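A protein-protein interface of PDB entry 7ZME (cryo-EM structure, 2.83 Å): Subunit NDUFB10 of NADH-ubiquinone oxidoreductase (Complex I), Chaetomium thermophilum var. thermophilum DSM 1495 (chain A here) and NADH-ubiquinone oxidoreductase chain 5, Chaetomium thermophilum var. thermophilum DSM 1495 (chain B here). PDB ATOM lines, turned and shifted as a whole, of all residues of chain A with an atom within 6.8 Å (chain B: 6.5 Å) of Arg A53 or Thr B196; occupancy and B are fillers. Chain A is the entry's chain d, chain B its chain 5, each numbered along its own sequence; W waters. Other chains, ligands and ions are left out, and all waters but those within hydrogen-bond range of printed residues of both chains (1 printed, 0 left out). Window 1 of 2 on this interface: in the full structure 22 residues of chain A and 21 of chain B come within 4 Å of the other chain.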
ATOM      1  N   VAL A  46       3.566  21.447 -19.174  1.00  0.00           N
ATOM      2  CA  VAL A  46       2.653  22.387 -18.542  1.00  0.00           C
ATOM      3  C   VAL A  46       2.375  23.565 -19.463  1.00  0.00           C
ATOM      4  O   VAL A  46       1.236  24.035 -19.563  1.00  0.00           O
ATOM      5  CB  VAL A  46       3.227  22.835 -17.189  1.00  0.00           C
ATOM      6  CG1 VAL A  46       2.444  24.011 -16.632  1.00  0.00           C
ATOM      7  CG2 VAL A  46       3.236  21.670 -16.230  1.00  0.00           C
ATOM      8  N   MET A  48       2.450  23.344 -22.590  1.00  0.00           N
ATOM      9  CA  MET A  48       1.561  22.768 -23.594  1.00  0.00           C
ATOM     10  C   MET A  48       0.109  22.929 -23.179  1.00  0.00           C
ATOM     11  O   MET A  48      -0.770  23.119 -24.028  1.00  0.00           O
ATOM     12  CB  MET A  48       1.902  21.293 -23.802  1.00  0.00           C
ATOM     13  CG  MET A  48       2.869  21.024 -24.940  1.00  0.00           C
ATOM     14  SD  MET A  48       3.436  19.321 -24.989  1.00  0.00           S
ATOM     15  CE  MET A  48       2.306  18.614 -26.178  1.00  0.00           C
ATOM     16  N   GLY A  49      -0.162  22.851 -21.876  1.00  0.00           N
ATOM     17  CA  GLY A  49      -1.502  23.130 -21.391  1.00  0.00           C
ATOM     18  C   GLY A  49      -1.921  24.570 -21.622  1.00  0.00           C
ATOM     19  O   GLY A  49      -3.050  24.836 -22.033  1.00  0.00           O
ATOM     20  N   ARG A  50      -1.016  25.518 -21.363  1.00  0.00           N
ATOM     21  CA  ARG A  50      -1.358  26.926 -21.534  1.00  0.00           C
ATOM     22  C   ARG A  50      -1.677  27.255 -22.983  1.00  0.00           C
ATOM     23  O   ARG A  50      -2.605  28.024 -23.258  1.00  0.00           O
ATOM     24  CB  ARG A  50      -0.232  27.820 -21.016  1.00  0.00           C
ATOM     25  CG  ARG A  50      -0.166  27.901 -19.503  1.00  0.00           C
ATOM     26  CD  ARG A  50       1.029  28.700 -19.027  1.00  0.00           C
ATOM     27  NE  ARG A  50       1.016  30.076 -19.506  1.00  0.00           N
ATOM     28  CZ  ARG A  50       2.001  30.944 -19.305  1.00  0.00           C
ATOM     29  NH1 ARG A  50       1.912  32.175 -19.782  1.00  0.00           N
ATOM     30  NH2 ARG A  50       3.068  30.587 -18.607  1.00  0.00           N
ATOM     31  N   LEU A  51      -0.920  26.694 -23.923  1.00  0.00           N
ATOM     32  CA  LEU A  51      -1.188  26.966 -25.328  1.00  0.00           C
ATOM     33  C   LEU A  51      -2.522  26.372 -25.755  1.00  0.00           C
ATOM     34  O   LEU A  51      -3.362  27.074 -26.319  1.00  0.00           O
ATOM     35  CB  LEU A  51      -0.053  26.429 -26.191  1.00  0.00           C
ATOM     36  CG  LEU A  51       1.225  27.258 -26.184  1.00  0.00           C
ATOM     37  CD1 LEU A  51       2.322  26.544 -26.949  1.00  0.00           C
ATOM     38  CD2 LEU A  51       0.957  28.630 -26.766  1.00  0.00           C
ATOM     39  N   VAL A  52      -2.748  25.090 -25.453  1.00  0.00           N
ATOM     40  CA  VAL A  52      -4.013  24.438 -25.791  1.00  0.00           C
ATOM     41  C   VAL A  52      -5.175  25.161 -25.131  1.00  0.00           C
ATOM     42  O   VAL A  52      -6.244  25.331 -25.730  1.00  0.00           O
ATOM     43  CB  VAL A  52      -3.974  22.951 -25.387  1.00  0.00           C
ATOM     44  CG1 VAL A  52      -5.364  22.337 -25.454  1.00  0.00           C
ATOM     45  CG2 VAL A  52      -3.014  22.187 -26.280  1.00  0.00           C
ATOM     46  N   ARG A  53      -4.983  25.601 -23.889  1.00  0.00           N
ATOM     47  CA  ARG A  53      -5.991  26.396 -23.203  1.00  0.00           C
ATOM     48  C   ARG A  53      -6.334  27.664 -23.968  1.00  0.00           C
ATOM     49  O   ARG A  53      -7.436  28.194 -23.808  1.00  0.00           O
ATOM     50  CB  ARG A  53      -5.496  26.734 -21.800  1.00  0.00           C
ATOM     51  CG  ARG A  53      -6.564  27.172 -20.839  1.00  0.00           C
ATOM     52  CD  ARG A  53      -5.967  28.010 -19.729  1.00  0.00           C
ATOM     53  NE  ARG A  53      -5.552  27.191 -18.596  1.00  0.00           N
ATOM     54  CZ  ARG A  53      -4.375  27.295 -17.993  1.00  0.00           C
ATOM     55  NH1 ARG A  53      -4.081  26.515 -16.964  1.00  0.00           N
ATOM     56  NH2 ARG A  53      -3.489  28.178 -18.424  1.00  0.00           N
ATOM     57  N   GLU A  54      -5.413  28.160 -24.793  1.00  0.00           N
ATOM     58  CA  GLU A  54      -5.638  29.407 -25.511  1.00  0.00           C
ATOM     59  C   GLU A  54      -6.487  29.208 -26.767  1.00  0.00           C
ATOM     60  O   GLU A  54      -7.283  30.088 -27.109  1.00  0.00           O
ATOM     61  CB  GLU A  54      -4.293  30.056 -25.842  1.00  0.00           C
ATOM     62  CG  GLU A  54      -4.396  31.416 -26.508  1.00  0.00           C
ATOM     63  CD  GLU A  54      -3.038  32.042 -26.765  1.00  0.00           C
ATOM     64  OE1 GLU A  54      -2.016  31.401 -26.445  1.00  0.00           O
ATOM     65  OE2 GLU A  54      -2.995  33.181 -27.276  1.00  0.00           O
ATOM     66  N   GLU A  55      -6.348  28.077 -27.475  1.00  0.00           N
ATOM     67  CA  GLU A  55      -7.263  27.845 -28.594  1.00  0.00           C
ATOM     68  C   GLU A  55      -8.644  27.451 -28.109  1.00  0.00           C
ATOM     69  O   GLU A  55      -9.641  27.746 -28.775  1.00  0.00           O
ATOM     70  CB  GLU A  55      -6.758  26.775 -29.570  1.00  0.00           C
ATOM     71  CG  GLU A  55      -5.518  27.140 -30.353  1.00  0.00           C
ATOM     72  CD  GLU A  55      -4.268  26.883 -29.583  1.00  0.00           C
ATOM     73  OE1 GLU A  55      -4.390  26.354 -28.472  1.00  0.00           O
ATOM     74  OE2 GLU A  55      -3.174  27.212 -30.078  1.00  0.00           O
ATOM     75  N   LEU A  56      -8.721  26.766 -26.972  1.00  0.00           N
ATOM     76  CA  LEU A  56     -10.018  26.461 -26.391  1.00  0.00           C
ATOM     77  C   LEU A  56     -10.722  27.735 -25.951  1.00  0.00           C
ATOM     78  O   LEU A  56     -11.950  27.839 -26.046  1.00  0.00           O
ATOM     79  CB  LEU A  56      -9.833  25.484 -25.232  1.00  0.00           C
ATOM     80  CG  LEU A  56     -11.038  24.845 -24.558  1.00  0.00           C
ATOM     81  CD1 LEU A  56     -10.630  23.510 -24.009  1.00  0.00           C
ATOM     82  CD2 LEU A  56     -11.504  25.719 -23.430  1.00  0.00           C
ATOM     83  N   SER A  57      -9.961  28.717 -25.471  1.00  0.00           N
ATOM     84  CA  SER A  57     -10.537  30.024 -25.181  1.00  0.00           C
ATOM     85  C   SER A  57     -11.014  30.709 -26.453  1.00  0.00           C
ATOM     86  O   SER A  57     -12.098  31.302 -26.478  1.00  0.00           O
ATOM     87  CB  SER A  57      -9.519  30.896 -24.454  1.00  0.00           C
ATOM     88  OG  SER A  57      -9.488  30.596 -23.073  1.00  0.00           O
ATOM     89  N   LYS A  58     -10.213  30.645 -27.520  1.00  0.00           N
ATOM     90  CA  LYS A  58     -10.610  31.260 -28.780  1.00  0.00           C
ATOM     91  C   LYS A  58     -11.810  30.550 -29.390  1.00  0.00           C
ATOM     92  O   LYS A  58     -12.707  31.198 -29.936  1.00  0.00           O
ATOM     93  CB  LYS A  58      -9.433  31.267 -29.753  1.00  0.00           C
ATOM     94  CG  LYS A  58      -8.509  32.458 -29.589  1.00  0.00           C
ATOM     95  CD  LYS A  58      -7.174  32.220 -30.273  1.00  0.00           C
ATOM     96  CE  LYS A  58      -6.551  33.527 -30.733  1.00  0.00           C
ATOM     97  NZ  LYS A  58      -5.197  33.321 -31.316  1.00  0.00           N
ATOM     98  N   TYR A  60     -14.160  28.988 -27.748  1.00  0.00           N
ATOM     99  CA  TYR A  60     -15.341  29.209 -26.919  1.00  0.00           C
ATOM    100  C   TYR A  60     -16.066  30.492 -27.306  1.00  0.00           C
ATOM    101  O   TYR A  60     -17.290  30.501 -27.475  1.00  0.00           O
ATOM    102  CB  TYR A  60     -14.931  29.244 -25.449  1.00  0.00           C
ATOM    103  CG  TYR A  60     -16.076  29.487 -24.507  1.00  0.00           C
ATOM    104  CD1 TYR A  60     -16.973  28.478 -24.215  1.00  0.00           C
ATOM    105  CD2 TYR A  60     -16.265  30.729 -23.919  1.00  0.00           C
ATOM    106  CE1 TYR A  60     -18.021  28.692 -23.363  1.00  0.00           C
ATOM    107  CE2 TYR A  60     -17.315  30.953 -23.063  1.00  0.00           C
ATOM    108  CZ  TYR A  60     -18.191  29.928 -22.788  1.00  0.00           C
ATOM    109  OH  TYR A  60     -19.245  30.130 -21.931  1.00  0.00           O
ATOM    110  N   TYR A  61     -15.328  31.591 -27.446  1.00  0.00           N
ATOM    111  CA  TYR A  61     -15.950  32.852 -27.822  1.00  0.00           C
ATOM    112  C   TYR A  61     -16.290  32.911 -29.302  1.00  0.00           C
ATOM    113  O   TYR A  61     -17.134  33.720 -29.700  1.00  0.00           O
ATOM    114  CB  TYR A  61     -15.040  34.019 -27.433  1.00  0.00           C
ATOM    115  CG  TYR A  61     -14.984  34.224 -25.940  1.00  0.00           C
ATOM    116  CD1 TYR A  61     -16.147  34.359 -25.203  1.00  0.00           C
ATOM    117  CD2 TYR A  61     -13.776  34.249 -25.265  1.00  0.00           C
ATOM    118  CE1 TYR A  61     -16.110  34.532 -23.843  1.00  0.00           C
ATOM    119  CE2 TYR A  61     -13.730  34.421 -23.903  1.00  0.00           C
ATOM    120  CZ  TYR A  61     -14.902  34.562 -23.197  1.00  0.00           C
ATOM    121  OH  TYR A  61     -14.871  34.735 -21.834  1.00  0.00           O
ATOM    122  N   LEU A  74     -10.233  20.162 -28.203  1.00  0.00           N
ATOM    123  CA  LEU A  74      -9.334  20.775 -27.237  1.00  0.00           C
ATOM    124  C   LEU A  74      -9.711  20.427 -25.803  1.00  0.00           C
ATOM    125  O   LEU A  74      -8.842  20.419 -24.926  1.00  0.00           O
ATOM    126  CB  LEU A  74      -9.324  22.290 -27.432  1.00  0.00           C
ATOM    127  CG  LEU A  74      -8.962  22.735 -28.847  1.00  0.00           C
ATOM    128  CD1 LEU A  74      -9.429  24.147 -29.111  1.00  0.00           C
ATOM    129  CD2 LEU A  74      -7.466  22.621 -29.060  1.00  0.00           C
ATOM    130  N   TYR A  78      -6.832  19.523 -23.528  1.00  0.00           N
ATOM    131  CA  TYR A  78      -6.501  20.248 -22.308  1.00  0.00           C
ATOM    132  C   TYR A  78      -6.662  19.366 -21.079  1.00  0.00           C
ATOM    133  O   TYR A  78      -5.833  19.412 -20.164  1.00  0.00           O
ATOM    134  CB  TYR A  78      -7.367  21.497 -22.168  1.00  0.00           C
ATOM    135  CG  TYR A  78      -7.176  22.197 -20.842  1.00  0.00           C
ATOM    136  CD1 TYR A  78      -6.063  22.986 -20.605  1.00  0.00           C
ATOM    137  CD2 TYR A  78      -8.097  22.046 -19.817  1.00  0.00           C
ATOM    138  CE1 TYR A  78      -5.880  23.613 -19.395  1.00  0.00           C
ATOM    139  CE2 TYR A  78      -7.923  22.666 -18.609  1.00  0.00           C
ATOM    140  CZ  TYR A  78      -6.815  23.451 -18.400  1.00  0.00           C
ATOM    141  OH  TYR A  78      -6.644  24.073 -17.186  1.00  0.00           O
ATOM    142  N   LEU A  82      -4.035  18.608 -18.376  1.00  0.00           N
ATOM    143  CA  LEU A  82      -4.314  19.049 -17.014  1.00  0.00           C
ATOM    144  C   LEU A  82      -4.099  17.923 -16.013  1.00  0.00           C
ATOM    145  O   LEU A  82      -3.607  18.159 -14.903  1.00  0.00           O
ATOM    146  CB  LEU A  82      -5.740  19.587 -16.919  1.00  0.00           C
ATOM    147  CG  LEU A  82      -6.235  20.022 -15.537  1.00  0.00           C
ATOM    148  CD1 LEU A  82      -5.454  21.222 -15.050  1.00  0.00           C
ATOM    149  CD2 LEU A  82      -7.724  20.323 -15.568  1.00  0.00           C
ATOM    150  N   GLU B  68       3.207  28.859 -13.272  1.00  0.00           N
ATOM    151  CA  GLU B  68       2.999  27.475 -13.770  1.00  0.00           C
ATOM    152  C   GLU B  68       1.646  27.399 -14.476  1.00  0.00           C
ATOM    153  O   GLU B  68       1.467  28.107 -15.476  1.00  0.00           O
ATOM    154  CB  GLU B  68       3.197  26.450 -12.654  1.00  0.00           C
ATOM    155  CG  GLU B  68       3.365  25.018 -13.126  1.00  0.00           C
ATOM    156  CD  GLU B  68       2.507  24.032 -12.352  1.00  0.00           C
ATOM    157  OE1 GLU B  68       1.444  24.442 -11.854  1.00  0.00           O
ATOM    158  OE2 GLU B  68       2.909  22.863 -12.236  1.00  0.00           O
ATOM    159  N   TRP B  69       0.753  26.539 -13.994  1.00  0.00           N
ATOM    160  CA  TRP B  69      -0.570  26.340 -14.627  1.00  0.00           C
ATOM    161  C   TRP B  69      -1.426  27.599 -14.595  1.00  0.00           C
ATOM    162  O   TRP B  69      -2.250  27.747 -15.500  1.00  0.00           O
ATOM    163  CB  TRP B  69      -1.307  25.189 -13.936  1.00  0.00           C
ATOM    164  CG  TRP B  69      -1.057  23.840 -14.531  1.00  0.00           C
ATOM    165  CD1 TRP B  69      -0.304  22.832 -14.003  1.00  0.00           C
ATOM    166  CD2 TRP B  69      -1.579  23.341 -15.773  1.00  0.00           C
ATOM    167  NE1 TRP B  69      -0.314  21.748 -14.835  1.00  0.00           N
ATOM    168  CE2 TRP B  69      -1.090  22.029 -15.927  1.00  0.00           C
ATOM    169  CE3 TRP B  69      -2.405  23.872 -16.765  1.00  0.00           C
ATOM    170  CZ2 TRP B  69      -1.400  21.250 -17.037  1.00  0.00           C
ATOM    171  CZ3 TRP B  69      -2.715  23.099 -17.859  1.00  0.00           C
ATOM    172  CH2 TRP B  69      -2.216  21.806 -17.992  1.00  0.00           C
ATOM    173  N   PHE B  70      -1.239  28.493 -13.618  1.00  0.00           N
ATOM    174  CA  PHE B  70      -2.207  29.578 -13.565  1.00  0.00           C
ATOM    175  C   PHE B  70      -1.669  30.773 -14.337  1.00  0.00           C
ATOM    176  O   PHE B  70      -0.571  31.260 -14.054  1.00  0.00           O
ATOM    177  CB  PHE B  70      -2.505  29.959 -12.116  1.00  0.00           C
ATOM    178  CG  PHE B  70      -2.842  28.790 -11.232  1.00  0.00           C
ATOM    179  CD1 PHE B  70      -3.350  27.616 -11.764  1.00  0.00           C
ATOM    180  CD2 PHE B  70      -2.650  28.864  -9.863  1.00  0.00           C
ATOM    181  CE1 PHE B  70      -3.652  26.546 -10.955  1.00  0.00           C
ATOM    182  CE2 PHE B  70      -2.956  27.794  -9.052  1.00  0.00           C
ATOM    183  CZ  PHE B  70      -3.457  26.637  -9.599  1.00  0.00           C
ATOM    184  N   ILE B  71      -2.440  31.239 -15.313  1.00  0.00           N
ATOM    185  CA  ILE B  71      -2.108  32.436 -16.081  1.00  0.00           C
ATOM    186  C   ILE B  71      -3.308  33.377 -16.008  1.00  0.00           C
ATOM    187  O   ILE B  71      -4.247  33.298 -16.804  1.00  0.00           O
ATOM    188  CB  ILE B  71      -1.691  32.124 -17.526  1.00  0.00           C
ATOM    189  CG1 ILE B  71      -1.193  33.390 -18.232  1.00  0.00           C
ATOM    190  CG2 ILE B  71      -2.750  31.334 -18.300  1.00  0.00           C
ATOM    191  CD1 ILE B  71       0.057  33.962 -17.655  1.00  0.00           C
ATOM    192  N   LEU B 189      -9.387  22.825 -12.157  1.00  0.00           N
ATOM    193  CA  LEU B 189      -9.268  23.178 -13.566  1.00  0.00           C
ATOM    194  C   LEU B 189      -7.909  23.718 -13.973  1.00  0.00           C
ATOM    195  O   LEU B 189      -7.628  23.765 -15.176  1.00  0.00           O
ATOM    196  CB  LEU B 189     -10.332  24.211 -13.968  1.00  0.00           C
ATOM    197  CG  LEU B 189     -11.742  23.722 -14.320  1.00  0.00           C
ATOM    198  CD1 LEU B 189     -11.711  22.833 -15.553  1.00  0.00           C
ATOM    199  CD2 LEU B 189     -12.438  23.038 -13.163  1.00  0.00           C
ATOM    200  N   GLY B 190      -7.064  24.137 -13.037  1.00  0.00           N
ATOM    201  CA  GLY B 190      -5.786  24.707 -13.394  1.00  0.00           C
ATOM    202  C   GLY B 190      -5.850  26.126 -13.905  1.00  0.00           C
ATOM    203  O   GLY B 190      -4.814  26.678 -14.291  1.00  0.00           O
ATOM    204  N   ASN B 191      -7.033  26.727 -13.931  1.00  0.00           N
ATOM    205  CA  ASN B 191      -7.205  28.121 -14.305  1.00  0.00           C
ATOM    206  C   ASN B 191      -8.597  28.551 -13.878  1.00  0.00           C
ATOM    207  O   ASN B 191      -9.421  27.737 -13.458  1.00  0.00           O
ATOM    208  CB  ASN B 191      -7.010  28.348 -15.805  1.00  0.00           C
ATOM    209  CG  ASN B 191      -6.268  29.629 -16.099  1.00  0.00           C
ATOM    210  OD1 ASN B 191      -5.282  29.951 -15.443  1.00  0.00           O
ATOM    211  ND2 ASN B 191      -6.747  30.375 -17.081  1.00  0.00           N
ATOM    212  N   LEU B 192      -8.847  29.849 -13.996  1.00  0.00           N
ATOM    213  CA  LEU B 192     -10.155  30.395 -13.664  1.00  0.00           C
ATOM    214  C   LEU B 192     -10.638  31.432 -14.677  1.00  0.00           C
ATOM    215  O   LEU B 192     -11.483  32.266 -14.338  1.00  0.00           O
ATOM    216  CB  LEU B 192     -10.123  30.924 -12.221  1.00  0.00           C
ATOM    217  CG  LEU B 192      -9.168  32.035 -11.789  1.00  0.00           C
ATOM    218  CD1 LEU B 192      -9.673  33.403 -12.096  1.00  0.00           C
ATOM    219  CD2 LEU B 192      -8.909  31.898 -10.298  1.00  0.00           C
ATOM    220  N   ASP B 193     -10.157  31.374 -15.916  1.00  0.00           N
ATOM    221  CA  ASP B 193     -10.770  32.117 -17.008  1.00  0.00           C
ATOM    222  C   ASP B 193     -12.177  31.603 -17.285  1.00  0.00           C
ATOM    223  O   ASP B 193     -12.454  30.408 -17.179  1.00  0.00           O
ATOM    224  CB  ASP B 193      -9.930  32.005 -18.279  1.00  0.00           C
ATOM    225  CG  ASP B 193      -8.634  32.772 -18.193  1.00  0.00           C
ATOM    226  OD1 ASP B 193      -8.595  33.795 -17.477  1.00  0.00           O
ATOM    227  OD2 ASP B 193      -7.655  32.359 -18.848  1.00  0.00           O
ATOM    228  N   TYR B 194     -13.066  32.521 -17.666  1.00  0.00           N
ATOM    229  CA  TYR B 194     -14.454  32.138 -17.912  1.00  0.00           C
ATOM    230  C   TYR B 194     -14.560  31.142 -19.057  1.00  0.00           C
ATOM    231  O   TYR B 194     -15.359  30.204 -18.999  1.00  0.00           O
ATOM    232  CB  TYR B 194     -15.304  33.376 -18.199  1.00  0.00           C
ATOM    233  CG  TYR B 194     -15.450  34.300 -17.018  1.00  0.00           C
ATOM    234  CD1 TYR B 194     -15.359  33.817 -15.723  1.00  0.00           C
ATOM    235  CD2 TYR B 194     -15.675  35.657 -17.196  1.00  0.00           C
ATOM    236  CE1 TYR B 194     -15.486  34.655 -14.643  1.00  0.00           C
ATOM    237  CE2 TYR B 194     -15.798  36.503 -16.121  1.00  0.00           C
ATOM    238  CZ  TYR B 194     -15.705  35.994 -14.847  1.00  0.00           C
ATOM    239  OH  TYR B 194     -15.833  36.826 -13.765  1.00  0.00           O
ATOM    240  N   ALA B 195     -13.760  31.331 -20.108  1.00  0.00           N
ATOM    241  CA  ALA B 195     -13.802  30.419 -21.244  1.00  0.00           C
ATOM    242  C   ALA B 195     -13.438  29.000 -20.829  1.00  0.00           C
ATOM    243  O   ALA B 195     -14.082  28.038 -21.258  1.00  0.00           O
ATOM    244  CB  ALA B 195     -12.864  30.911 -22.345  1.00  0.00           C
ATOM    245  N   THR B 196     -12.415  28.851 -19.992  1.00  0.00           N
ATOM    246  CA  THR B 196     -11.973  27.519 -19.599  1.00  0.00           C
ATOM    247  C   THR B 196     -12.904  26.900 -18.566  1.00  0.00           C
ATOM    248  O   THR B 196     -13.131  25.688 -18.581  1.00  0.00           O
ATOM    249  CB  THR B 196     -10.550  27.581 -19.052  1.00  0.00           C
ATOM    250  OG1 THR B 196     -10.568  28.159 -17.743  1.00  0.00           O
ATOM    251  CG2 THR B 196      -9.699  28.454 -19.947  1.00  0.00           C
ATOM    252  N   VAL B 197     -13.445  27.717 -17.662  1.00  0.00           N
ATOM    253  CA  VAL B 197     -14.314  27.201 -16.609  1.00  0.00           C
ATOM    254  C   VAL B 197     -15.635  26.714 -17.189  1.00  0.00           C
ATOM    255  O   VAL B 197     -16.161  25.674 -16.780  1.00  0.00           O
ATOM    256  CB  VAL B 197     -14.528  28.274 -15.524  1.00  0.00           C
ATOM    257  CG1 VAL B 197     -15.578  27.831 -14.537  1.00  0.00           C
ATOM    258  CG2 VAL B 197     -13.235  28.549 -14.794  1.00  0.00           C
ATOM    259  N   PHE B 198     -16.183  27.438 -18.158  1.00  0.00           N
ATOM    260  CA  PHE B 198     -17.522  27.142 -18.647  1.00  0.00           C
ATOM    261  C   PHE B 198     -17.530  26.131 -19.782  1.00  0.00           C
ATOM    262  O   PHE B 198     -18.532  25.433 -19.971  1.00  0.00           O
ATOM    263  CB  PHE B 198     -18.208  28.433 -19.098  1.00  0.00           C
ATOM    264  CG  PHE B 198     -18.284  29.478 -18.025  1.00  0.00           C
ATOM    265  CD1 PHE B 198     -18.290  29.117 -16.692  1.00  0.00           C
ATOM    266  CD2 PHE B 198     -18.346  30.816 -18.350  1.00  0.00           C
ATOM    267  CE1 PHE B 198     -18.354  30.066 -15.710  1.00  0.00           C
ATOM    268  CE2 PHE B 198     -18.409  31.771 -17.365  1.00  0.00           C
ATOM    269  CZ  PHE B 198     -18.412  31.395 -16.045  1.00  0.00           C
ATOM    270  N   SER B 199     -16.438  26.036 -20.539  1.00  0.00           N
ATOM    271  CA  SER B 199     -16.344  25.006 -21.565  1.00  0.00           C
ATOM    272  C   SER B 199     -16.231  23.620 -20.948  1.00  0.00           C
ATOM    273  O   SER B 199     -16.769  22.648 -21.487  1.00  0.00           O
ATOM    274  CB  SER B 199     -15.148  25.283 -22.465  1.00  0.00           C
ATOM    275  OG  SER B 199     -13.986  25.434 -21.677  1.00  0.00           O
ATOM    276  N   LEU B 200     -15.539  23.510 -19.820  1.00  0.00           N
ATOM    277  CA  LEU B 200     -15.283  22.219 -19.203  1.00  0.00           C
ATOM    278  C   LEU B 200     -16.286  21.848 -18.122  1.00  0.00           C
ATOM    279  O   LEU B 200     -16.292  20.694 -17.686  1.00  0.00           O
ATOM    280  CB  LEU B 200     -13.873  22.197 -18.614  1.00  0.00           C
ATOM    281  CG  LEU B 200     -12.776  22.196 -19.678  1.00  0.00           C
ATOM    282  CD1 LEU B 200     -11.490  22.774 -19.125  1.00  0.00           C
ATOM    283  CD2 LEU B 200     -12.563  20.804 -20.224  1.00  0.00           C
ATOM    284  N   ALA B 201     -17.144  22.780 -17.705  1.00  0.00           N
ATOM    285  CA  ALA B 201     -18.037  22.529 -16.575  1.00  0.00           C
ATOM    286  C   ALA B 201     -18.934  21.302 -16.727  1.00  0.00           C
ATOM    287  O   ALA B 201     -19.096  20.575 -15.733  1.00  0.00           O
ATOM    288  CB  ALA B 201     -18.883  23.779 -16.302  1.00  0.00           C
ATOM    289  N   ILE B 204     -17.219  17.959 -15.504  1.00  0.00           N
ATOM    290  CA  ILE B 204     -16.498  17.981 -14.245  1.00  0.00           C
ATOM    291  C   ILE B 204     -17.334  17.276 -13.184  1.00  0.00           C
ATOM    292  O   ILE B 204     -18.559  17.192 -13.285  1.00  0.00           O
ATOM    293  CB  ILE B 204     -16.168  19.437 -13.856  1.00  0.00           C
ATOM    294  CG1 ILE B 204     -15.254  20.054 -14.900  1.00  0.00           C
ATOM    295  CG2 ILE B 204     -15.419  19.513 -12.565  1.00  0.00           C
ATOM    296  CD1 ILE B 204     -15.098  21.522 -14.739  1.00  0.00           C
HETATM  297  O   HOH W   1     -12.734  34.284 -20.401  1.00  0.00           O
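The backbone carbonyl oxygen (O) of Arg A53 is in hydrogen-bond range of the side-chain hydroxyl (OG) of Ser A57 (3.2 Å).
The backbone NH (N) of Ile B71 sits at hydrogen-bond distance from the side-chain amide oxygen (OD1) of Asn B191.
The side-chain amide nitrogen (ND2) of Asn B191 is in hydrogen-bond range of the side-chain carboxylate (OD2) of Asp B193 (2.8 Å).
O of Asp B193 sits at hydrogen-bond distance from OG1 of Thr B196, 3.0 Å away.
The backbone carbonyl oxygen of Ala B195 is in hydrogen-bond range of the side-chain hydroxyl of Ser B199.
The side-chain hydroxyl of Ser B199 lies within hydrogen-bond range of the backbone carbonyl oxygen of Thr B196.
Of the 18 printed residues of chain B, 12 touch a printed residue of chain A.
Among the printed residues, no Asp or Glu carboxylate lies within 4 Å of a Lys or Arg side-chain nitrogen of the other chain.
Arg A53 touches just these residues of chain B: Trp B69, Ile B71, Gly B190, Asn B191 and Thr B196.
Printed residues of chain A within 4 Å of Thr B196: Arg A53 and Ser A57.
Printed residues of chain A within 4 Å of Trp B69: Val A46 (3.8 Å), Gly A49 (3.7 Å), Arg A53 (2.6 Å), Tyr A78 (3.6 Å) and Leu A82 (3.6 Å).
Of the printed residues of chain B, Tyr A61 touches Tyr B194 and Ala B195.
Of the printed residues of chain A, Tyr B194 touches Tyr A61 (3.9 Å).
NH1 of Arg A53 is in hydrogen-bond range of O of Trp B69 (2.6 Å).
The guanidinium group of Arg A53 is in hydrogen-bond range of the backbone carbonyl oxygen of Gly B190 (2.8 Å).
The side-chain hydroxyl (OH) of Tyr A78 sits close to the backbone carbonyl oxygen (O) of Leu B189 (2.3 Å).
Water W1 lies within hydrogen-bond range of OH of Tyr A61 (2.6 Å), N of Ala B195 (3.1 Å) and N of Tyr B194 (3.3 Å).
CG1 of Val A46 touches CG of Glu B68, at 3.8 Å.
Val A46 touches Trp B69 (CG2 to NE1, 3.8 Å).
CA of Gly A49 touches CH2 of Trp B69, 3.7 Å away.
Ser B199 touches Leu A56.
Ala B195 touches Ser A57 (CB to OG, 3.5 Å).
CG2 of Thr B196 touches OG of Ser A57 (3.8 Å).
CB of Phe B198 touches OH of Tyr A60 (3.5 Å).
OH of Tyr A61 touches CB of Tyr B194, 3.9 Å away.
CE1 of Tyr A78 touches CZ3 of Trp B69, 3.6 Å away.
Gly B190 touches Leu A82.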
